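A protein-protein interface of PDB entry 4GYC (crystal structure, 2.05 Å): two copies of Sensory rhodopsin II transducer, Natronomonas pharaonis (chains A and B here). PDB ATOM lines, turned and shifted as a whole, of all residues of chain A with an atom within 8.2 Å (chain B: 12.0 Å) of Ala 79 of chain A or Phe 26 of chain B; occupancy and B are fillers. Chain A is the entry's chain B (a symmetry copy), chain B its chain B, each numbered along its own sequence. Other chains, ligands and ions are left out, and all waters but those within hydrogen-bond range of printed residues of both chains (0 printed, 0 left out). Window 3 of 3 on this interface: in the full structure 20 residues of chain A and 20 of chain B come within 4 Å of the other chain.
The side-chain hydroxyl of Thr 33 of chain B lies within hydrogen-bond range of the backbone carbonyl oxygen of Val 29 of chain B (2.7 Å).
OG1 of Thr 33 of chain B lies within hydrogen-bond range of ND2 of Asn 74 of chain B (3.0 Å).
The backbone carbonyl oxygen of Leu 70 of chain B lies close to the side-chain amide nitrogen of Asn 74 of chain B, 3.4 Å away.
Among the printed residues, merely in contact across the chains: Phe 26 of chain A with Ala 79 of chain B (3.4 Å), Leu 71 of chain A with Thr 33 of chain B (2.9 Å), Leu 71 of chain A with Leu 71 of chain B (3.7 Å), Leu 71 of chain A with Asn 74 of chain B (3.9 Å), Asn 74 of chain A with Leu 71 of chain B (3.9 Å), Leu 75 of chain A with Val 29 of chain B (3.4 Å), Leu 75 of chain A with Val 78 of chain B (3.8 Å), Val 78 of chain A with Leu 75 of chain B (3.8 Å) and Ala 79 of chain A with Phe 26 of chain B (3.4 Å).
Of chain B, only Phe 26 comes within 4 Å of Ala 79 of chain A.
Of the printed residues of chain A, Phe 26 of chain B touches Ala 79.
No residue of chain B comes within 4 Å of Gly 76 of chain A.
Leu 77 of chain A touches none of the printed residues of chain B.
Val 78 of chain A touches one residue of chain B.
No residue of chain B comes within 4 Å of Thr 81 of chain A.
No residue of chain B comes within 4 Å of Leu 82 of chain A.
No residue of chain B comes within 4 Å of Gly 83 of chain A.
No residue of chain A comes within 4 Å of Val 25 of chain B.
Printed residues of chain A within 4 Å of Leu 71 of chain B: Leu 71 and Asn 74.
Of the printed residues of chain A, Ala 79 of chain B touches Phe 26 (3.4 Å).
Of the printed residues of chain A, Asn 74 of chain B touches Leu 71.
Printed residues of chain B within 4 Å of Asn 74 of chain A: Leu 71 (3.9 Å).
The nearest residue of chain A that does not touch Phe 26 of chain B is Leu 75 of chain A (4.1 Å).
The nearest printed residue of chain A that does not touch Leu 71 of chain B is Leu 75 of chain A (5.6 Å).
Of the 27 printed residues of chain B, 8 touch a printed residue of chain A.
Printed residues of chain B that touch a printed residue of chain A: Phe 26, Val 29, Thr 33, Leu 71, Asn 74, Leu 75, Val 78 and Ala 79.
Of the 15 printed residues of chain A, 6 touch a printed residue of chain B.
Hydrophobic or aromatic side chains of chain A that line the printed part of chain B: Phe 26, Leu 71, Leu 75, Val 78 and Ala 79.
Phe 26 of chain A touches Ala 79 of chain B, and with the chains exchanged Ala 79 of chain A touches Phe 26 of chain B.
Leu 71 of chain A touches its own counterpart, Leu 71 of chain B.
Leu 71 of chain A touches Asn 74 of chain B, and with the chains exchanged Asn 74 of chain A touches Leu 71 of chain B.
Leu 75 of chain A touches Val 78 of chain B, and with the chains exchanged Val 78 of chain A touches Leu 75 of chain B.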
ATOM      1  N   VAL A  25       6.455  10.624  -3.503  1.00  0.00           N
ATOM      2  CA  VAL A  25       6.598  10.679  -2.056  1.00  0.00           C
ATOM      3  C   VAL A  25       8.057  10.881  -1.690  1.00  0.00           C
ATOM      4  O   VAL A  25       8.371  11.483  -0.662  1.00  0.00           O
ATOM      5  CB  VAL A  25       6.076   9.388  -1.378  1.00  0.00           C
ATOM      6  CG1 VAL A  25       6.866   8.178  -1.856  1.00  0.00           C
ATOM      7  CG2 VAL A  25       6.161   9.504   0.138  1.00  0.00           C
ATOM      8  N   PHE A  26       8.947  10.382  -2.542  1.00  0.00           N
ATOM      9  CA  PHE A  26      10.377  10.483  -2.290  1.00  0.00           C
ATOM     10  C   PHE A  26      10.912  11.895  -2.526  1.00  0.00           C
ATOM     11  O   PHE A  26      11.885  12.307  -1.893  1.00  0.00           O
ATOM     12  CB  PHE A  26      11.155   9.465  -3.127  1.00  0.00           C
ATOM     13  CG  PHE A  26      11.091   8.067  -2.585  1.00  0.00           C
ATOM     14  CD1 PHE A  26      11.958   7.657  -1.590  1.00  0.00           C
ATOM     15  CD2 PHE A  26      10.167   7.162  -3.074  1.00  0.00           C
ATOM     16  CE1 PHE A  26      11.903   6.376  -1.088  1.00  0.00           C
ATOM     17  CE2 PHE A  26      10.112   5.879  -2.574  1.00  0.00           C
ATOM     18  CZ  PHE A  26      10.984   5.487  -1.581  1.00  0.00           C
ATOM     19  N   LEU A  71      14.142  11.674  10.124  1.00  0.00           N
ATOM     20  CA  LEU A  71      14.306  10.396   9.433  1.00  0.00           C
ATOM     21  C   LEU A  71      13.187   9.423   9.783  1.00  0.00           C
ATOM     22  O   LEU A  71      12.627   8.764   8.907  1.00  0.00           O
ATOM     23  CB  LEU A  71      15.658   9.742   9.758  1.00  0.00           C
ATOM     24  CG  LEU A  71      15.594   8.249   9.375  1.00  0.00           C
ATOM     25  CD1 LEU A  71      15.704   8.042   7.853  1.00  0.00           C
ATOM     26  CD2 LEU A  71      16.631   7.391  10.111  1.00  0.00           C
ATOM     27  N   GLY A  72      12.868   9.314  11.068  1.00  0.00           N
ATOM     28  CA  GLY A  72      11.789   8.432  11.472  1.00  0.00           C
ATOM     29  C   GLY A  72      10.481   8.800  10.787  1.00  0.00           C
ATOM     30  O   GLY A  72       9.746   7.928  10.291  1.00  0.00           O
ATOM     31  N   ILE A  73      10.183  10.100  10.759  1.00  0.00           N
ATOM     32  CA  ILE A  73       8.949  10.571  10.151  1.00  0.00           C
ATOM     33  C   ILE A  73       8.932  10.222   8.669  1.00  0.00           C
ATOM     34  O   ILE A  73       7.944   9.694   8.160  1.00  0.00           O
ATOM     35  CB  ILE A  73       8.760  12.099  10.302  1.00  0.00           C
ATOM     36  CG1 ILE A  73       8.652  12.494  11.794  1.00  0.00           C
ATOM     37  CG2 ILE A  73       7.546  12.556   9.470  1.00  0.00           C
ATOM     38  CD1 ILE A  73       8.704  13.999  12.050  1.00  0.00           C
ATOM     39  N   ASN A  74      10.016  10.534   7.967  1.00  0.00           N
ATOM     40  CA  ASN A  74      10.072  10.231   6.542  1.00  0.00           C
ATOM     41  C   ASN A  74       9.957   8.730   6.240  1.00  0.00           C
ATOM     42  O   ASN A  74       9.301   8.336   5.285  1.00  0.00           O
ATOM     43  CB  ASN A  74      11.347  10.796   5.931  1.00  0.00           C
ATOM     44  CG  ASN A  74      11.363  12.317   5.946  1.00  0.00           C
ATOM     45  OD1 ASN A  74      10.317  12.954   6.020  1.00  0.00           O
ATOM     46  ND2 ASN A  74      12.545  12.897   5.866  1.00  0.00           N
ATOM     47  N   LEU A  75      10.611   7.910   7.056  1.00  0.00           N
ATOM     48  CA  LEU A  75      10.586   6.460   6.875  1.00  0.00           C
ATOM     49  C   LEU A  75       9.201   5.915   7.159  1.00  0.00           C
ATOM     50  O   LEU A  75       8.709   5.032   6.448  1.00  0.00           O
ATOM     51  CB  LEU A  75      11.600   5.785   7.793  1.00  0.00           C
ATOM     52  CG  LEU A  75      13.059   5.807   7.349  1.00  0.00           C
ATOM     53  CD1 LEU A  75      13.924   5.212   8.443  1.00  0.00           C
ATOM     54  CD2 LEU A  75      13.239   5.046   6.047  1.00  0.00           C
ATOM     55  N   GLY A  76       8.575   6.449   8.202  1.00  0.00           N
ATOM     56  CA  GLY A  76       7.221   6.074   8.549  1.00  0.00           C
ATOM     57  C   GLY A  76       6.282   6.371   7.398  1.00  0.00           C
ATOM     58  O   GLY A  76       5.460   5.534   7.020  1.00  0.00           O
ATOM     59  N   LEU A  77       6.410   7.569   6.837  1.00  0.00           N
ATOM     60  CA  LEU A  77       5.618   7.964   5.683  1.00  0.00           C
ATOM     61  C   LEU A  77       5.846   7.020   4.489  1.00  0.00           C
ATOM     62  O   LEU A  77       4.891   6.546   3.871  1.00  0.00           O
ATOM     63  CB  LEU A  77       5.926   9.413   5.296  1.00  0.00           C
ATOM     64  CG  LEU A  77       5.310   9.943   3.994  1.00  0.00           C
ATOM     65  CD1 LEU A  77       3.804   9.715   3.955  1.00  0.00           C
ATOM     66  CD2 LEU A  77       5.638  11.422   3.816  1.00  0.00           C
ATOM     67  N   VAL A  78       7.110   6.746   4.182  1.00  0.00           N
ATOM     68  CA  VAL A  78       7.475   5.882   3.062  1.00  0.00           C
ATOM     69  C   VAL A  78       6.999   4.436   3.253  1.00  0.00           C
ATOM     70  O   VAL A  78       6.425   3.824   2.343  1.00  0.00           O
ATOM     71  CB  VAL A  78       9.008   5.876   2.840  1.00  0.00           C
ATOM     72  CG1 VAL A  78       9.425   4.682   1.967  1.00  0.00           C
ATOM     73  CG2 VAL A  78       9.462   7.193   2.217  1.00  0.00           C
ATOM     74  N   ALA A  79       7.267   3.894   4.436  1.00  0.00           N
ATOM     75  CA  ALA A  79       6.881   2.532   4.759  1.00  0.00           C
ATOM     76  C   ALA A  79       5.370   2.423   4.650  1.00  0.00           C
ATOM     77  O   ALA A  79       4.840   1.493   4.041  1.00  0.00           O
ATOM     78  CB  ALA A  79       7.348   2.167   6.172  1.00  0.00           C
ATOM     79  N   ALA A  80       4.686   3.402   5.226  1.00  0.00           N
ATOM     80  CA  ALA A  80       3.233   3.401   5.279  1.00  0.00           C
ATOM     81  C   ALA A  80       2.560   3.482   3.918  1.00  0.00           C
ATOM     82  O   ALA A  80       1.488   2.916   3.727  1.00  0.00           O
ATOM     83  CB  ALA A  80       2.737   4.521   6.176  1.00  0.00           C
ATOM     84  N   THR A  81       3.163   4.194   2.972  1.00  0.00           N
ATOM     85  CA  THR A  81       2.525   4.356   1.663  1.00  0.00           C
ATOM     86  C   THR A  81       2.991   3.347   0.624  1.00  0.00           C
ATOM     87  O   THR A  81       2.240   2.991  -0.284  1.00  0.00           O
ATOM     88  CB  THR A  81       2.702   5.782   1.094  1.00  0.00           C
ATOM     89  OG1 THR A  81       4.093   6.134   1.073  1.00  0.00           O
ATOM     90  CG2 THR A  81       1.947   6.779   1.942  1.00  0.00           C
ATOM     91  N   LEU A  82       4.224   2.878   0.755  1.00  0.00           N
ATOM     92  CA  LEU A  82       4.785   1.983  -0.253  1.00  0.00           C
ATOM     93  C   LEU A  82       5.052   0.571   0.268  1.00  0.00           C
ATOM     94  O   LEU A  82       5.239  -0.357  -0.517  1.00  0.00           O
ATOM     95  CB  LEU A  82       6.048   2.594  -0.867  1.00  0.00           C
ATOM     96  CG  LEU A  82       5.839   3.654  -1.961  1.00  0.00           C
ATOM     97  CD1 LEU A  82       4.691   4.606  -1.650  1.00  0.00           C
ATOM     98  CD2 LEU A  82       7.121   4.433  -2.201  1.00  0.00           C
ATOM     99  N   GLY A  83       5.056   0.408   1.586  1.00  0.00           N
ATOM    100  CA  GLY A  83       5.201  -0.905   2.187  1.00  0.00           C
ATOM    101  C   GLY A  83       3.987  -1.779   1.921  1.00  0.00           C
ATOM    102  O   GLY A  83       3.026  -1.343   1.285  1.00  0.00           O
ATOM    103  N   GLY B  23      11.330  -5.912   6.672  1.00  0.00           N
ATOM    104  CA  GLY B  23      10.896  -5.343   7.941  1.00  0.00           C
ATOM    105  C   GLY B  23      12.022  -5.107   8.939  1.00  0.00           C
ATOM    106  O   GLY B  23      11.914  -4.261   9.829  1.00  0.00           O
ATOM    107  N   ALA B  24      13.104  -5.865   8.797  1.00  0.00           N
ATOM    108  CA  ALA B  24      14.272  -5.693   9.645  1.00  0.00           C
ATOM    109  C   ALA B  24      15.131  -4.557   9.104  1.00  0.00           C
ATOM    110  O   ALA B  24      15.868  -3.911   9.849  1.00  0.00           O
ATOM    111  CB  ALA B  24      15.074  -6.975   9.700  1.00  0.00           C
ATOM    112  N   VAL B  25      15.025  -4.325   7.799  1.00  0.00           N
ATOM    113  CA  VAL B  25      15.780  -3.272   7.137  1.00  0.00           C
ATOM    114  C   VAL B  25      15.555  -1.951   7.850  1.00  0.00           C
ATOM    115  O   VAL B  25      16.430  -1.084   7.863  1.00  0.00           O
ATOM    116  CB  VAL B  25      15.377  -3.123   5.649  1.00  0.00           C
ATOM    117  CG1 VAL B  25      13.905  -2.756   5.530  1.00  0.00           C
ATOM    118  CG2 VAL B  25      16.237  -2.073   4.960  1.00  0.00           C
ATOM    119  N   PHE B  26      14.378  -1.806   8.451  1.00  0.00           N
ATOM    120  CA  PHE B  26      14.027  -0.574   9.144  1.00  0.00           C
ATOM    121  C   PHE B  26      14.752  -0.431  10.481  1.00  0.00           C
ATOM    122  O   PHE B  26      15.015   0.685  10.931  1.00  0.00           O
ATOM    123  CB  PHE B  26      12.514  -0.465   9.335  1.00  0.00           C
ATOM    124  CG  PHE B  26      11.777  -0.056   8.095  1.00  0.00           C
ATOM    125  CD1 PHE B  26      11.658   1.279   7.755  1.00  0.00           C
ATOM    126  CD2 PHE B  26      11.200  -1.003   7.270  1.00  0.00           C
ATOM    127  CE1 PHE B  26      10.985   1.661   6.615  1.00  0.00           C
ATOM    128  CE2 PHE B  26      10.524  -0.623   6.131  1.00  0.00           C
ATOM    129  CZ  PHE B  26      10.417   0.712   5.805  1.00  0.00           C
ATOM    130  N   ILE B  27      15.075  -1.554  11.117  1.00  0.00           N
ATOM    131  CA  ILE B  27      15.817  -1.502  12.372  1.00  0.00           C
ATOM    132  C   ILE B  27      17.306  -1.329  12.103  1.00  0.00           C
ATOM    133  O   ILE B  27      18.026  -0.745  12.912  1.00  0.00           O
ATOM    134  CB  ILE B  27      15.558  -2.735  13.272  1.00  0.00           C
ATOM    135  CG1 ILE B  27      16.327  -3.964  12.768  1.00  0.00           C
ATOM    136  CG2 ILE B  27      14.061  -2.992  13.402  1.00  0.00           C
ATOM    137  CD1 ILE B  27      17.697  -4.149  13.416  1.00  0.00           C
ATOM    138  N   PHE B  28      17.764  -1.834  10.961  1.00  0.00           N
ATOM    139  CA  PHE B  28      19.133  -1.582  10.538  1.00  0.00           C
ATOM    140  C   PHE B  28      19.333  -0.083  10.300  1.00  0.00           C
ATOM    141  O   PHE B  28      20.298   0.517  10.769  1.00  0.00           O
ATOM    142  CB  PHE B  28      19.457  -2.365   9.268  1.00  0.00           C
ATOM    143  CG  PHE B  28      20.835  -2.098   8.730  1.00  0.00           C
ATOM    144  CD1 PHE B  28      21.946  -2.710   9.298  1.00  0.00           C
ATOM    145  CD2 PHE B  28      21.023  -1.234   7.667  1.00  0.00           C
ATOM    146  CE1 PHE B  28      23.217  -2.465   8.812  1.00  0.00           C
ATOM    147  CE2 PHE B  28      22.291  -0.986   7.174  1.00  0.00           C
ATOM    148  CZ  PHE B  28      23.391  -1.606   7.747  1.00  0.00           C
ATOM    149  N   VAL B  29      18.397   0.509   9.568  1.00  0.00           N
ATOM    150  CA  VAL B  29      18.455   1.921   9.224  1.00  0.00           C
ATOM    151  C   VAL B  29      18.308   2.820  10.454  1.00  0.00           C
ATOM    152  O   VAL B  29      19.064   3.787  10.629  1.00  0.00           O
ATOM    153  CB  VAL B  29      17.387   2.251   8.173  1.00  0.00           C
ATOM    154  CG1 VAL B  29      17.007   3.695   8.241  1.00  0.00           C
ATOM    155  CG2 VAL B  29      17.886   1.865   6.790  1.00  0.00           C
ATOM    156  N   GLY B  30      17.357   2.487  11.320  1.00  0.00           N
ATOM    157  CA  GLY B  30      17.122   3.267  12.525  1.00  0.00           C
ATOM    158  C   GLY B  30      18.281   3.237  13.505  1.00  0.00           C
ATOM    159  O   GLY B  30      18.601   4.250  14.131  1.00  0.00           O
ATOM    160  N   ALA B  31      18.908   2.073  13.646  1.00  0.00           N
ATOM    161  CA  ALA B  31      20.044   1.916  14.551  1.00  0.00           C
ATOM    162  C   ALA B  31      21.299   2.564  13.976  1.00  0.00           C
ATOM    163  O   ALA B  31      22.082   3.173  14.698  1.00  0.00           O
ATOM    164  CB  ALA B  31      20.292   0.443  14.843  1.00  0.00           C
ATOM    165  N   LEU B  32      21.521   2.418  12.669  1.00  0.00           N
ATOM    166  CA  LEU B  32      22.668   3.068  12.028  1.00  0.00           C
ATOM    167  C   LEU B  32      22.569   4.592  12.147  1.00  0.00           C
ATOM    168  O   LEU B  32      23.574   5.282  12.323  1.00  0.00           O
ATOM    169  CB  LEU B  32      22.771   2.682  10.552  1.00  0.00           C
ATOM    170  CG  LEU B  32      24.035   1.926  10.134  1.00  0.00           C
ATOM    171  CD1 LEU B  32      25.263   2.522  10.762  1.00  0.00           C
ATOM    172  CD2 LEU B  32      23.941   0.444  10.484  1.00  0.00           C
ATOM    173  N   THR B  33      21.350   5.108  12.057  1.00  0.00           N
ATOM    174  CA  THR B  33      21.119   6.538  12.173  1.00  0.00           C
ATOM    175  C   THR B  33      21.502   7.085  13.557  1.00  0.00           C
ATOM    176  O   THR B  33      22.093   8.164  13.667  1.00  0.00           O
ATOM    177  CB  THR B  33      19.651   6.875  11.847  1.00  0.00           C
ATOM    178  OG1 THR B  33      19.357   6.424  10.513  1.00  0.00           O
ATOM    179  CG2 THR B  33      19.419   8.378  11.929  1.00  0.00           C
ATOM    180  N   VAL B  34      21.177   6.341  14.607  1.00  0.00           N
ATOM    181  CA  VAL B  34      21.538   6.775  15.949  1.00  0.00           C
ATOM    182  C   VAL B  34      23.052   6.682  16.147  1.00  0.00           C
ATOM    183  O   VAL B  34      23.661   7.537  16.789  1.00  0.00           O
ATOM    184  CB  VAL B  34      20.786   5.975  17.040  1.00  0.00           C
ATOM    185  CG1 VAL B  34      19.273   6.117  16.858  1.00  0.00           C
ATOM    186  CG2 VAL B  34      21.194   4.516  17.010  1.00  0.00           C
ATOM    187  N   LEU B  35      23.662   5.653  15.570  1.00  0.00           N
ATOM    188  CA  LEU B  35      25.109   5.505  15.638  1.00  0.00           C
ATOM    189  C   LEU B  35      25.776   6.694  14.948  1.00  0.00           C
ATOM    190  O   LEU B  35      26.713   7.302  15.484  1.00  0.00           O
ATOM    191  CB  LEU B  35      25.540   4.192  14.987  1.00  0.00           C
ATOM    192  CG  LEU B  35      26.985   3.735  15.206  1.00  0.00           C
ATOM    193  CD1 LEU B  35      27.171   2.299  14.717  1.00  0.00           C
ATOM    194  CD2 LEU B  35      27.992   4.669  14.539  1.00  0.00           C
ATOM    195  N   LEU B  70      22.778  10.902   4.901  1.00  0.00           N
ATOM    196  CA  LEU B  70      22.391   9.646   5.519  1.00  0.00           C
ATOM    197  C   LEU B  70      20.922   9.319   5.237  1.00  0.00           C
ATOM    198  O   LEU B  70      20.583   8.175   4.965  1.00  0.00           O
ATOM    199  CB  LEU B  70      22.646   9.658   7.029  1.00  0.00           C
ATOM    200  CG  LEU B  70      22.499   8.275   7.696  1.00  0.00           C
ATOM    201  CD1 LEU B  70      23.679   7.389   7.358  1.00  0.00           C
ATOM    202  CD2 LEU B  70      22.371   8.368   9.198  1.00  0.00           C
ATOM    203  N   LEU B  71      20.046  10.317   5.291  1.00  0.00           N
ATOM    204  CA  LEU B  71      18.656  10.079   4.908  1.00  0.00           C
ATOM    205  C   LEU B  71      18.550   9.541   3.488  1.00  0.00           C
ATOM    206  O   LEU B  71      17.810   8.593   3.225  1.00  0.00           O
ATOM    207  CB  LEU B  71      17.807  11.356   5.024  1.00  0.00           C
ATOM    208  CG  LEU B  71      16.508  11.166   4.214  1.00  0.00           C
ATOM    209  CD1 LEU B  71      15.500  10.264   4.950  1.00  0.00           C
ATOM    210  CD2 LEU B  71      15.849  12.490   3.808  1.00  0.00           C
ATOM    211  N   GLY B  72      19.277  10.153   2.558  1.00  0.00           N
ATOM    212  CA  GLY B  72      19.253   9.674   1.188  1.00  0.00           C
ATOM    213  C   GLY B  72      19.678   8.215   1.102  1.00  0.00           C
ATOM    214  O   GLY B  72      19.048   7.401   0.403  1.00  0.00           O
ATOM    215  N   ILE B  73      20.756   7.877   1.812  1.00  0.00           N
ATOM    216  CA  ILE B  73      21.270   6.517   1.790  1.00  0.00           C
ATOM    217  C   ILE B  73      20.226   5.557   2.343  1.00  0.00           C
ATOM    218  O   ILE B  73      19.947   4.520   1.744  1.00  0.00           O
ATOM    219  CB  ILE B  73      22.571   6.364   2.611  1.00  0.00           C
ATOM    220  CG1 ILE B  73      23.704   7.233   2.017  1.00  0.00           C
ATOM    221  CG2 ILE B  73      22.948   4.872   2.712  1.00  0.00           C
ATOM    222  CD1 ILE B  73      24.949   7.330   2.896  1.00  0.00           C
ATOM    223  N   ASN B  74      19.662   5.887   3.502  1.00  0.00           N
ATOM    224  CA  ASN B  74      18.655   5.015   4.094  1.00  0.00           C
ATOM    225  C   ASN B  74      17.413   4.840   3.209  1.00  0.00           C
ATOM    226  O   ASN B  74      16.866   3.750   3.112  1.00  0.00           O
ATOM    227  CB  ASN B  74      18.254   5.530   5.469  1.00  0.00           C
ATOM    228  CG  ASN B  74      19.397   5.441   6.469  1.00  0.00           C
ATOM    229  OD1 ASN B  74      20.325   4.657   6.292  1.00  0.00           O
ATOM    230  ND2 ASN B  74      19.326   6.233   7.521  1.00  0.00           N
ATOM    231  N   LEU B  75      16.975   5.927   2.582  1.00  0.00           N
ATOM    232  CA  LEU B  75      15.800   5.896   1.713  1.00  0.00           C
ATOM    233  C   LEU B  75      16.085   5.082   0.466  1.00  0.00           C
ATOM    234  O   LEU B  75      15.238   4.311   0.004  1.00  0.00           O
ATOM    235  CB  LEU B  75      15.384   7.309   1.318  1.00  0.00           C
ATOM    236  CG  LEU B  75      14.592   8.111   2.345  1.00  0.00           C
ATOM    237  CD1 LEU B  75      14.388   9.522   1.830  1.00  0.00           C
ATOM    238  CD2 LEU B  75      13.258   7.447   2.638  1.00  0.00           C
ATOM    239  N   GLY B  76      17.286   5.259  -0.075  1.00  0.00           N
ATOM    240  CA  GLY B  76      17.720   4.497  -1.226  1.00  0.00           C
ATOM    241  C   GLY B  76      17.699   3.016  -0.915  1.00  0.00           C
ATOM    242  O   GLY B  76      17.192   2.212  -1.699  1.00  0.00           O
ATOM    243  N   LEU B  77      18.249   2.655   0.240  1.00  0.00           N
ATOM    244  CA  LEU B  77      18.243   1.274   0.695  1.00  0.00           C
ATOM    245  C   LEU B  77      16.810   0.730   0.835  1.00  0.00           C
ATOM    246  O   LEU B  77      16.501  -0.358   0.346  1.00  0.00           O
ATOM    247  CB  LEU B  77      19.004   1.146   2.018  1.00  0.00           C
ATOM    248  CG  LEU B  77      18.951  -0.211   2.735  1.00  0.00           C
ATOM    249  CD1 LEU B  77      19.350  -1.350   1.805  1.00  0.00           C
ATOM    250  CD2 LEU B  77      19.838  -0.191   3.975  1.00  0.00           C
ATOM    251  N   VAL B  78      15.946   1.498   1.492  1.00  0.00           N
ATOM    252  CA  VAL B  78      14.558   1.099   1.717  1.00  0.00           C
ATOM    253  C   VAL B  78      13.761   0.973   0.413  1.00  0.00           C
ATOM    254  O   VAL B  78      13.043  -0.010   0.192  1.00  0.00           O
ATOM    255  CB  VAL B  78      13.834   2.104   2.647  1.00  0.00           C
ATOM    256  CG1 VAL B  78      12.311   1.931   2.551  1.00  0.00           C
ATOM    257  CG2 VAL B  78      14.313   1.939   4.086  1.00  0.00           C
ATOM    258  N   ALA B  79      13.879   1.990  -0.434  1.00  0.00           N
ATOM    259  CA  ALA B  79      13.179   2.013  -1.706  1.00  0.00           C
ATOM    260  C   ALA B  79      13.632   0.815  -2.523  1.00  0.00           C
ATOM    261  O   ALA B  79      12.818   0.086  -3.091  1.00  0.00           O
ATOM    262  CB  ALA B  79      13.474   3.318  -2.454  1.00  0.00           C
ATOM    263  N   ALA B  80      14.942   0.608  -2.552  1.00  0.00           N
ATOM    264  CA  ALA B  80      15.539  -0.447  -3.355  1.00  0.00           C
ATOM    265  C   ALA B  80      15.140  -1.852  -2.931  1.00  0.00           C
ATOM    266  O   ALA B  80      15.034  -2.741  -3.771  1.00  0.00           O
ATOM    267  CB  ALA B  80      17.052  -0.312  -3.362  1.00  0.00           C
ATOM    268  N   THR B  81      14.935  -2.073  -1.637  1.00  0.00           N
ATOM    269  CA  THR B  81      14.610  -3.423  -1.169  1.00  0.00           C
ATOM    270  C   THR B  81      13.117  -3.683  -1.029  1.00  0.00           C
ATOM    271  O   THR B  81      12.662  -4.816  -1.177  1.00  0.00           O
ATOM    272  CB  THR B  81      15.308  -3.768   0.165  1.00  0.00           C
ATOM    273  OG1 THR B  81      15.016  -2.765   1.148  1.00  0.00           O
ATOM    274  CG2 THR B  81      16.804  -3.852  -0.035  1.00  0.00           C
ATOM    275  N   LEU B  82      12.351  -2.637  -0.751  1.00  0.00           N
ATOM    276  CA  LEU B  82      10.924  -2.812  -0.502  1.00  0.00           C
ATOM    277  C   LEU B  82      10.036  -2.166  -1.566  1.00  0.00           C
ATOM    278  O   LEU B  82       8.849  -2.473  -1.656  1.00  0.00           O
ATOM    279  CB  LEU B  82      10.560  -2.312   0.900  1.00  0.00           C
ATOM    280  CG  LEU B  82      10.856  -3.264   2.069  1.00  0.00           C
ATOM    281  CD1 LEU B  82      12.186  -3.992   1.918  1.00  0.00           C
ATOM    282  CD2 LEU B  82      10.811  -2.517   3.391  1.00  0.00           C
ATOM    283  N   GLY B  83      10.614  -1.285  -2.376  1.00  0.00           N
ATOM    284  CA  GLY B  83       9.890  -0.686  -3.482  1.00  0.00           C
ATOM    285  C   GLY B  83       9.569  -1.708  -4.559  1.00  0.00           C
ATOM    286  O   GLY B  83       9.935  -2.878  -4.444  1.00  0.00           O
